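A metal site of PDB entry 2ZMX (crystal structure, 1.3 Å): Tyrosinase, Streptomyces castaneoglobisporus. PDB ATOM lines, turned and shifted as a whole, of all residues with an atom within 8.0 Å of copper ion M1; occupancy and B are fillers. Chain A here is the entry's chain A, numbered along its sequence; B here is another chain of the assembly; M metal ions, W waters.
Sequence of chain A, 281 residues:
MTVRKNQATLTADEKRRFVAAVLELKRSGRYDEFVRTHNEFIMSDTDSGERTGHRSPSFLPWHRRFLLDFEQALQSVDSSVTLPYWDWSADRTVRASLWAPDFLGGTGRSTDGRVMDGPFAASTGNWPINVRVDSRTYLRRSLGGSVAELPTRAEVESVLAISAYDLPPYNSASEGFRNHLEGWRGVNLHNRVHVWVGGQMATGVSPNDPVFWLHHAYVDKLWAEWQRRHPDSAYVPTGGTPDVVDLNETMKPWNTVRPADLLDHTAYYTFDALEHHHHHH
A ring nitrogen (NE2) of His 215 is in hydrogen-bond range of the backbone carbonyl oxygen (O) of His 190 (3.1 Å).
The side-chain amide oxygen of Asn 191 lies within hydrogen-bond range of a ring nitrogen (ND1) of His 190 (2.9 Å).
A ring nitrogen (ND1) of His 190 is in hydrogen-bond range of the backbone carbonyl oxygen (O) of Glu 182 (3.1 Å).
ND1 of His 194 sits at hydrogen-bond distance from O of Met 201 (2.7 Å).
The side-chain hydroxyl (OH) of Tyr 98 of chain B lies within hydrogen-bond range of the side-chain hydroxyl (OG) of Ser 206 (3.0 Å).
Merely in contact with copper ion M1: Tyr 98 of chain B (3.95 Å).
Four residues have an atom within 4 Å of copper ion M1: His 190, His 194, His 216 and Tyr 98 of chain B.
The nearest printed residue that does not touch copper ion M1 is Phe 212 (4.2 Å).
Copper ion M1 is bound by water W1, a ring nitrogen (NE2) of His 190, a ring nitrogen (NE2) of His 194 and a ring nitrogen (NE2) of His 216.
Copper ion M1 has four donor atoms within binding distance.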
ATOM      1  N   HIS A  38      30.529  -7.328  -8.258  1.00  0.00           N
ATOM      2  CA  HIS A  38      30.202  -8.634  -7.706  1.00  0.00           C
ATOM      3  C   HIS A  38      29.213  -9.407  -8.585  1.00  0.00           C
ATOM      4  O   HIS A  38      29.367 -10.599  -8.846  1.00  0.00           O
ATOM      5  CB  HIS A  38      29.632  -8.463  -6.286  1.00  0.00           C
ATOM      6  CG  HIS A  38      29.460  -9.805  -5.611  1.00  0.00           C
ATOM      7  ND1 HIS A  38      28.266 -10.468  -5.560  1.00  0.00           N
ATOM      8  CD2 HIS A  38      30.357 -10.615  -4.977  1.00  0.00           C
ATOM      9  CE1 HIS A  38      28.396 -11.609  -4.923  1.00  0.00           C
ATOM     10  NE2 HIS A  38      29.652 -11.717  -4.554  1.00  0.00           N
ATOM     11  N   ILE A  42      29.475 -13.073 -10.340  1.00  0.00           N
ATOM     12  CA  ILE A  42      28.676 -14.229  -9.969  1.00  0.00           C
ATOM     13  C   ILE A  42      27.835 -14.738 -11.133  1.00  0.00           C
ATOM     14  O   ILE A  42      27.548 -15.933 -11.250  1.00  0.00           O
ATOM     15  CB  ILE A  42      27.852 -13.822  -8.747  1.00  0.00           C
ATOM     16  CG1 ILE A  42      27.594 -15.040  -7.841  1.00  0.00           C
ATOM     17  CG2 ILE A  42      26.595 -13.093  -9.170  1.00  0.00           C
ATOM     18  CD1 ILE A  42      27.253 -14.594  -6.436  1.00  0.00           C
ATOM     19  N   GLY A  53      35.498 -15.688  -9.131  1.00  0.00           N
ATOM     20  CA  GLY A  53      35.082 -15.132  -7.830  1.00  0.00           C
ATOM     21  C   GLY A  53      34.385 -16.130  -6.947  1.00  0.00           C
ATOM     22  O   GLY A  53      34.367 -15.930  -5.720  1.00  0.00           O
ATOM     23  N   HIS A  54      33.827 -17.181  -7.502  1.00  0.00           N
ATOM     24  CA  HIS A  54      32.954 -18.135  -6.815  1.00  0.00           C
ATOM     25  C   HIS A  54      33.163 -19.509  -7.389  1.00  0.00           C
ATOM     26  O   HIS A  54      33.716 -19.685  -8.464  1.00  0.00           O
ATOM     27  CB  HIS A  54      31.443 -17.792  -7.024  1.00  0.00           C
ATOM     28  CG  HIS A  54      31.143 -16.377  -6.605  1.00  0.00           C
ATOM     29  ND1 HIS A  54      31.398 -15.299  -7.453  1.00  0.00           N
ATOM     30  CD2 HIS A  54      30.691 -15.910  -5.420  1.00  0.00           C
ATOM     31  CE1 HIS A  54      31.058 -14.210  -6.745  1.00  0.00           C
ATOM     32  NE2 HIS A  54      30.631 -14.552  -5.549  1.00  0.00           N
ATOM     33  N   PHE A  59      37.640 -18.448  -4.843  1.00  0.00           N
ATOM     34  CA  PHE A  59      36.577 -17.859  -4.040  1.00  0.00           C
ATOM     35  C   PHE A  59      37.100 -17.144  -2.803  1.00  0.00           C
ATOM     36  O   PHE A  59      36.698 -15.994  -2.549  1.00  0.00           O
ATOM     37  CB  PHE A  59      35.599 -18.966  -3.635  1.00  0.00           C
ATOM     38  CG  PHE A  59      34.563 -18.586  -2.557  1.00  0.00           C
ATOM     39  CD1 PHE A  59      33.528 -17.691  -2.829  1.00  0.00           C
ATOM     40  CD2 PHE A  59      34.660 -19.141  -1.298  1.00  0.00           C
ATOM     41  CE1 PHE A  59      32.607 -17.384  -1.851  1.00  0.00           C
ATOM     42  CE2 PHE A  59      33.720 -18.823  -0.315  1.00  0.00           C
ATOM     43  CZ  PHE A  59      32.679 -17.953  -0.599  1.00  0.00           C
ATOM     44  N   HIS A  63      37.488 -12.945  -2.693  1.00  0.00           N
ATOM     45  CA  HIS A  63      36.682 -12.172  -1.762  1.00  0.00           C
ATOM     46  C   HIS A  63      37.566 -11.442  -0.749  1.00  0.00           C
ATOM     47  O   HIS A  63      37.209 -10.338  -0.270  1.00  0.00           O
ATOM     48  CB  HIS A  63      35.622 -13.042  -1.059  1.00  0.00           C
ATOM     49  CG  HIS A  63      34.429 -13.251  -1.922  1.00  0.00           C
ATOM     50  ND1 HIS A  63      34.344 -14.264  -2.867  1.00  0.00           N
ATOM     51  CD2 HIS A  63      33.271 -12.569  -2.031  1.00  0.00           C
ATOM     52  CE1 HIS A  63      33.166 -14.191  -3.517  1.00  0.00           C
ATOM     53  NE2 HIS A  63      32.479 -13.165  -3.005  1.00  0.00           N
ATOM     54  N   GLU A 182      32.303 -22.641   1.193  1.00  0.00           N
ATOM     55  CA  GLU A 182      31.373 -21.943   0.287  1.00  0.00           C
ATOM     56  C   GLU A 182      29.959 -22.445   0.414  1.00  0.00           C
ATOM     57  O   GLU A 182      28.984 -21.667   0.476  1.00  0.00           O
ATOM     58  CB  GLU A 182      31.942 -22.045  -1.144  1.00  0.00           C
ATOM     59  CG  GLU A 182      31.270 -21.090  -2.096  1.00  0.00           C
ATOM     60  CD  GLU A 182      31.757 -21.066  -3.506  1.00  0.00           C
ATOM     61  OE1 GLU A 182      32.829 -21.683  -3.760  1.00  0.00           O
ATOM     62  OE2 GLU A 182      31.136 -20.419  -4.381  1.00  0.00           O
ATOM     63  N   HIS A 190      28.556 -20.790   3.887  1.00  0.00           N
ATOM     64  CA  HIS A 190      28.400 -19.454   3.314  1.00  0.00           C
ATOM     65  C   HIS A 190      27.147 -19.260   2.486  1.00  0.00           C
ATOM     66  O   HIS A 190      26.469 -18.219   2.585  1.00  0.00           O
ATOM     67  CB  HIS A 190      29.666 -19.118   2.480  1.00  0.00           C
ATOM     68  CG  HIS A 190      29.420 -18.178   1.328  1.00  0.00           C
ATOM     69  ND1 HIS A 190      29.026 -18.609   0.097  1.00  0.00           N
ATOM     70  CD2 HIS A 190      29.560 -16.848   1.229  1.00  0.00           C
ATOM     71  CE1 HIS A 190      28.889 -17.567  -0.735  1.00  0.00           C
ATOM     72  NE2 HIS A 190      29.208 -16.471  -0.034  1.00  0.00           N
ATOM     73  N   ASN A 191      26.798 -20.243   1.612  1.00  0.00           N
ATOM     74  CA  ASN A 191      25.599 -20.049   0.805  1.00  0.00           C
ATOM     75  C   ASN A 191      24.357 -19.972   1.688  1.00  0.00           C
ATOM     76  O   ASN A 191      23.455 -19.167   1.428  1.00  0.00           O
ATOM     77  CB  ASN A 191      25.390 -21.184  -0.202  1.00  0.00           C
ATOM     78  CG  ASN A 191      26.397 -21.147  -1.346  1.00  0.00           C
ATOM     79  OD1 ASN A 191      27.151 -20.193  -1.501  1.00  0.00           O
ATOM     80  ND2 ASN A 191      26.381 -22.200  -2.160  1.00  0.00           N
ATOM     81  N   VAL A 193      24.034 -18.834   4.673  1.00  0.00           N
ATOM     82  CA  VAL A 193      23.789 -17.522   5.297  1.00  0.00           C
ATOM     83  C   VAL A 193      23.161 -16.551   4.318  1.00  0.00           C
ATOM     84  O   VAL A 193      22.264 -15.784   4.716  1.00  0.00           O
ATOM     85  CB  VAL A 193      25.111 -16.973   5.823  1.00  0.00           C
ATOM     86  CG1 VAL A 193      24.904 -15.568   6.398  1.00  0.00           C
ATOM     87  CG2 VAL A 193      25.668 -17.906   6.881  1.00  0.00           C
ATOM     88  N   HIS A 194      23.615 -16.530   3.052  1.00  0.00           N
ATOM     89  CA  HIS A 194      22.943 -15.682   2.089  1.00  0.00           C
ATOM     90  C   HIS A 194      21.447 -15.974   1.989  1.00  0.00           C
ATOM     91  O   HIS A 194      20.576 -15.085   1.906  1.00  0.00           O
ATOM     92  CB  HIS A 194      23.543 -15.837   0.683  1.00  0.00           C
ATOM     93  CG  HIS A 194      24.824 -15.117   0.410  1.00  0.00           C
ATOM     94  ND1 HIS A 194      24.852 -13.790  -0.028  1.00  0.00           N
ATOM     95  CD2 HIS A 194      26.111 -15.543   0.430  1.00  0.00           C
ATOM     96  CE1 HIS A 194      26.121 -13.482  -0.207  1.00  0.00           C
ATOM     97  NE2 HIS A 194      26.968 -14.495   0.032  1.00  0.00           N
ATOM     98  N   MET A 201      20.368  -9.927  -0.373  1.00  0.00           N
ATOM     99  CA  MET A 201      21.460 -10.832   0.025  1.00  0.00           C
ATOM    100  C   MET A 201      21.329 -12.217  -0.567  1.00  0.00           C
ATOM    101  O   MET A 201      22.356 -12.921  -0.644  1.00  0.00           O
ATOM    102  CB  MET A 201      21.447 -10.857   1.555  1.00  0.00           C
ATOM    103  CG  MET A 201      22.647 -11.417   2.216  1.00  0.00           C
ATOM    104  SD  MET A 201      24.248 -10.687   1.821  1.00  0.00           S
ATOM    105  CE  MET A 201      25.204 -11.790   2.905  1.00  0.00           C
ATOM    106  N   THR A 203      20.484 -12.839  -3.659  1.00  0.00           N
ATOM    107  CA  THR A 203      20.589 -12.647  -5.104  1.00  0.00           C
ATOM    108  C   THR A 203      21.993 -12.344  -5.588  1.00  0.00           C
ATOM    109  O   THR A 203      22.927 -12.198  -4.800  1.00  0.00           O
ATOM    110  CB  THR A 203      19.668 -11.503  -5.593  1.00  0.00           C
ATOM    111  OG1 THR A 203      20.306 -10.259  -5.221  1.00  0.00           O
ATOM    112  CG2 THR A 203      18.305 -11.620  -4.947  1.00  0.00           C
ATOM    113  N   SER A 206      23.949  -9.209  -4.099  1.00  0.00           N
ATOM    114  CA  SER A 206      23.936  -9.265  -2.640  1.00  0.00           C
ATOM    115  C   SER A 206      24.759  -8.183  -1.944  1.00  0.00           C
ATOM    116  O   SER A 206      24.352  -7.873  -0.809  1.00  0.00           O
ATOM    117  CB  SER A 206      24.425 -10.657  -2.173  1.00  0.00           C
ATOM    118  OG  SER A 206      25.668 -11.003  -2.760  1.00  0.00           O
ATOM    119  N   PRO A 207      25.811  -7.580  -2.486  1.00  0.00           N
ATOM    120  CA  PRO A 207      26.405  -6.440  -1.746  1.00  0.00           C
ATOM    121  C   PRO A 207      25.454  -5.253  -1.611  1.00  0.00           C
ATOM    122  O   PRO A 207      25.826  -4.319  -0.870  1.00  0.00           O
ATOM    123  CB  PRO A 207      27.628  -6.063  -2.607  1.00  0.00           C
ATOM    124  CG  PRO A 207      27.964  -7.390  -3.269  1.00  0.00           C
ATOM    125  CD  PRO A 207      26.605  -7.890  -3.691  1.00  0.00           C
ATOM    126  N   PHE A 212      26.478  -7.945   3.712  1.00  0.00           N
ATOM    127  CA  PHE A 212      27.368  -8.718   2.868  1.00  0.00           C
ATOM    128  C   PHE A 212      28.808  -8.723   3.359  1.00  0.00           C
ATOM    129  O   PHE A 212      29.509  -9.722   3.328  1.00  0.00           O
ATOM    130  CB  PHE A 212      27.331  -8.101   1.445  1.00  0.00           C
ATOM    131  CG  PHE A 212      28.256  -8.728   0.444  1.00  0.00           C
ATOM    132  CD1 PHE A 212      29.573  -8.284   0.256  1.00  0.00           C
ATOM    133  CD2 PHE A 212      27.815  -9.804  -0.333  1.00  0.00           C
ATOM    134  CE1 PHE A 212      30.416  -8.910  -0.614  1.00  0.00           C
ATOM    135  CE2 PHE A 212      28.692 -10.404  -1.227  1.00  0.00           C
ATOM    136  CZ  PHE A 212      29.999  -9.965  -1.363  1.00  0.00           C
ATOM    137  N   HIS A 215      29.313 -10.683   6.677  1.00  0.00           N
ATOM    138  CA  HIS A 215      29.294 -12.114   6.359  1.00  0.00           C
ATOM    139  C   HIS A 215      30.640 -12.517   5.764  1.00  0.00           C
ATOM    140  O   HIS A 215      31.319 -13.434   6.272  1.00  0.00           O
ATOM    141  CB  HIS A 215      28.139 -12.381   5.393  1.00  0.00           C
ATOM    142  CG  HIS A 215      28.077 -13.799   4.883  1.00  0.00           C
ATOM    143  ND1 HIS A 215      28.443 -14.842   5.686  1.00  0.00           N
ATOM    144  CD2 HIS A 215      27.692 -14.295   3.680  1.00  0.00           C
ATOM    145  CE1 HIS A 215      28.279 -15.967   4.990  1.00  0.00           C
ATOM    146  NE2 HIS A 215      27.839 -15.673   3.785  1.00  0.00           N
ATOM    147  N   HIS A 216      31.066 -11.852   4.670  1.00  0.00           N
ATOM    148  CA  HIS A 216      32.310 -12.271   4.048  1.00  0.00           C
ATOM    149  C   HIS A 216      33.507 -12.002   4.936  1.00  0.00           C
ATOM    150  O   HIS A 216      34.496 -12.773   4.784  1.00  0.00           O
ATOM    151  CB  HIS A 216      32.453 -11.612   2.652  1.00  0.00           C
ATOM    152  CG  HIS A 216      31.794 -12.511   1.644  1.00  0.00           C
ATOM    153  ND1 HIS A 216      32.452 -13.610   1.101  1.00  0.00           N
ATOM    154  CD2 HIS A 216      30.564 -12.530   1.084  1.00  0.00           C
ATOM    155  CE1 HIS A 216      31.625 -14.241   0.270  1.00  0.00           C
ATOM    156  NE2 HIS A 216      30.460 -13.603   0.226  1.00  0.00           N
ATOM    157  N   VAL A 219      33.578 -15.251   6.850  1.00  0.00           N
ATOM    158  CA  VAL A 219      34.076 -16.322   5.980  1.00  0.00           C
ATOM    159  C   VAL A 219      35.563 -16.215   5.844  1.00  0.00           C
ATOM    160  O   VAL A 219      36.292 -17.232   5.852  1.00  0.00           O
ATOM    161  CB  VAL A 219      33.372 -16.243   4.614  1.00  0.00           C
ATOM    162  CG1 VAL A 219      33.990 -17.162   3.556  1.00  0.00           C
ATOM    163  CG2 VAL A 219      31.889 -16.557   4.759  1.00  0.00           C
ATOM    164  N   HIS B  97      20.511 -17.000  -6.006  1.00  0.00           N
ATOM    165  CA  HIS B  97      21.772 -17.458  -6.588  1.00  0.00           C
ATOM    166  C   HIS B  97      22.411 -18.496  -5.697  1.00  0.00           C
ATOM    167  O   HIS B  97      23.274 -19.273  -6.121  1.00  0.00           O
ATOM    168  CB  HIS B  97      22.713 -16.259  -6.775  1.00  0.00           C
ATOM    169  CG  HIS B  97      24.005 -16.779  -7.328  1.00  0.00           C
ATOM    170  ND1 HIS B  97      24.118 -16.967  -8.685  1.00  0.00           N
ATOM    171  CD2 HIS B  97      25.196 -17.150  -6.805  1.00  0.00           C
ATOM    172  CE1 HIS B  97      25.304 -17.429  -8.975  1.00  0.00           C
ATOM    173  NE2 HIS B  97      25.978 -17.553  -7.858  1.00  0.00           N
ATOM    174  N   TYR B  98      22.047 -18.519  -4.427  1.00  0.00           N
ATOM    175  CA  TYR B  98      22.823 -19.369  -3.501  1.00  0.00           C
ATOM    176  C   TYR B  98      22.009 -20.569  -3.063  1.00  0.00           C
ATOM    177  O   TYR B  98      22.281 -21.199  -2.038  1.00  0.00           O
ATOM    178  CB  TYR B  98      23.278 -18.526  -2.308  1.00  0.00           C
ATOM    179  CG  TYR B  98      24.046 -17.268  -2.639  1.00  0.00           C
ATOM    180  CD1 TYR B  98      23.440 -16.029  -2.814  1.00  0.00           C
ATOM    181  CD2 TYR B  98      25.442 -17.307  -2.788  1.00  0.00           C
ATOM    182  CE1 TYR B  98      24.149 -14.881  -3.115  1.00  0.00           C
ATOM    183  CE2 TYR B  98      26.128 -16.161  -3.089  1.00  0.00           C
ATOM    184  CZ  TYR B  98      25.511 -14.953  -3.260  1.00  0.00           C
ATOM    185  OH  TYR B  98      26.252 -13.807  -3.541  1.00  0.00           O
HETATM  186 CU    CU M   1      28.853 -14.607  -0.674  1.00  0.00          CU
HETATM  187 CU    CU M   2      30.290 -13.475  -3.911  1.00  0.00          CU
HETATM  188  O   HOH W   1      28.774 -13.565  -2.309  1.00  0.00           O
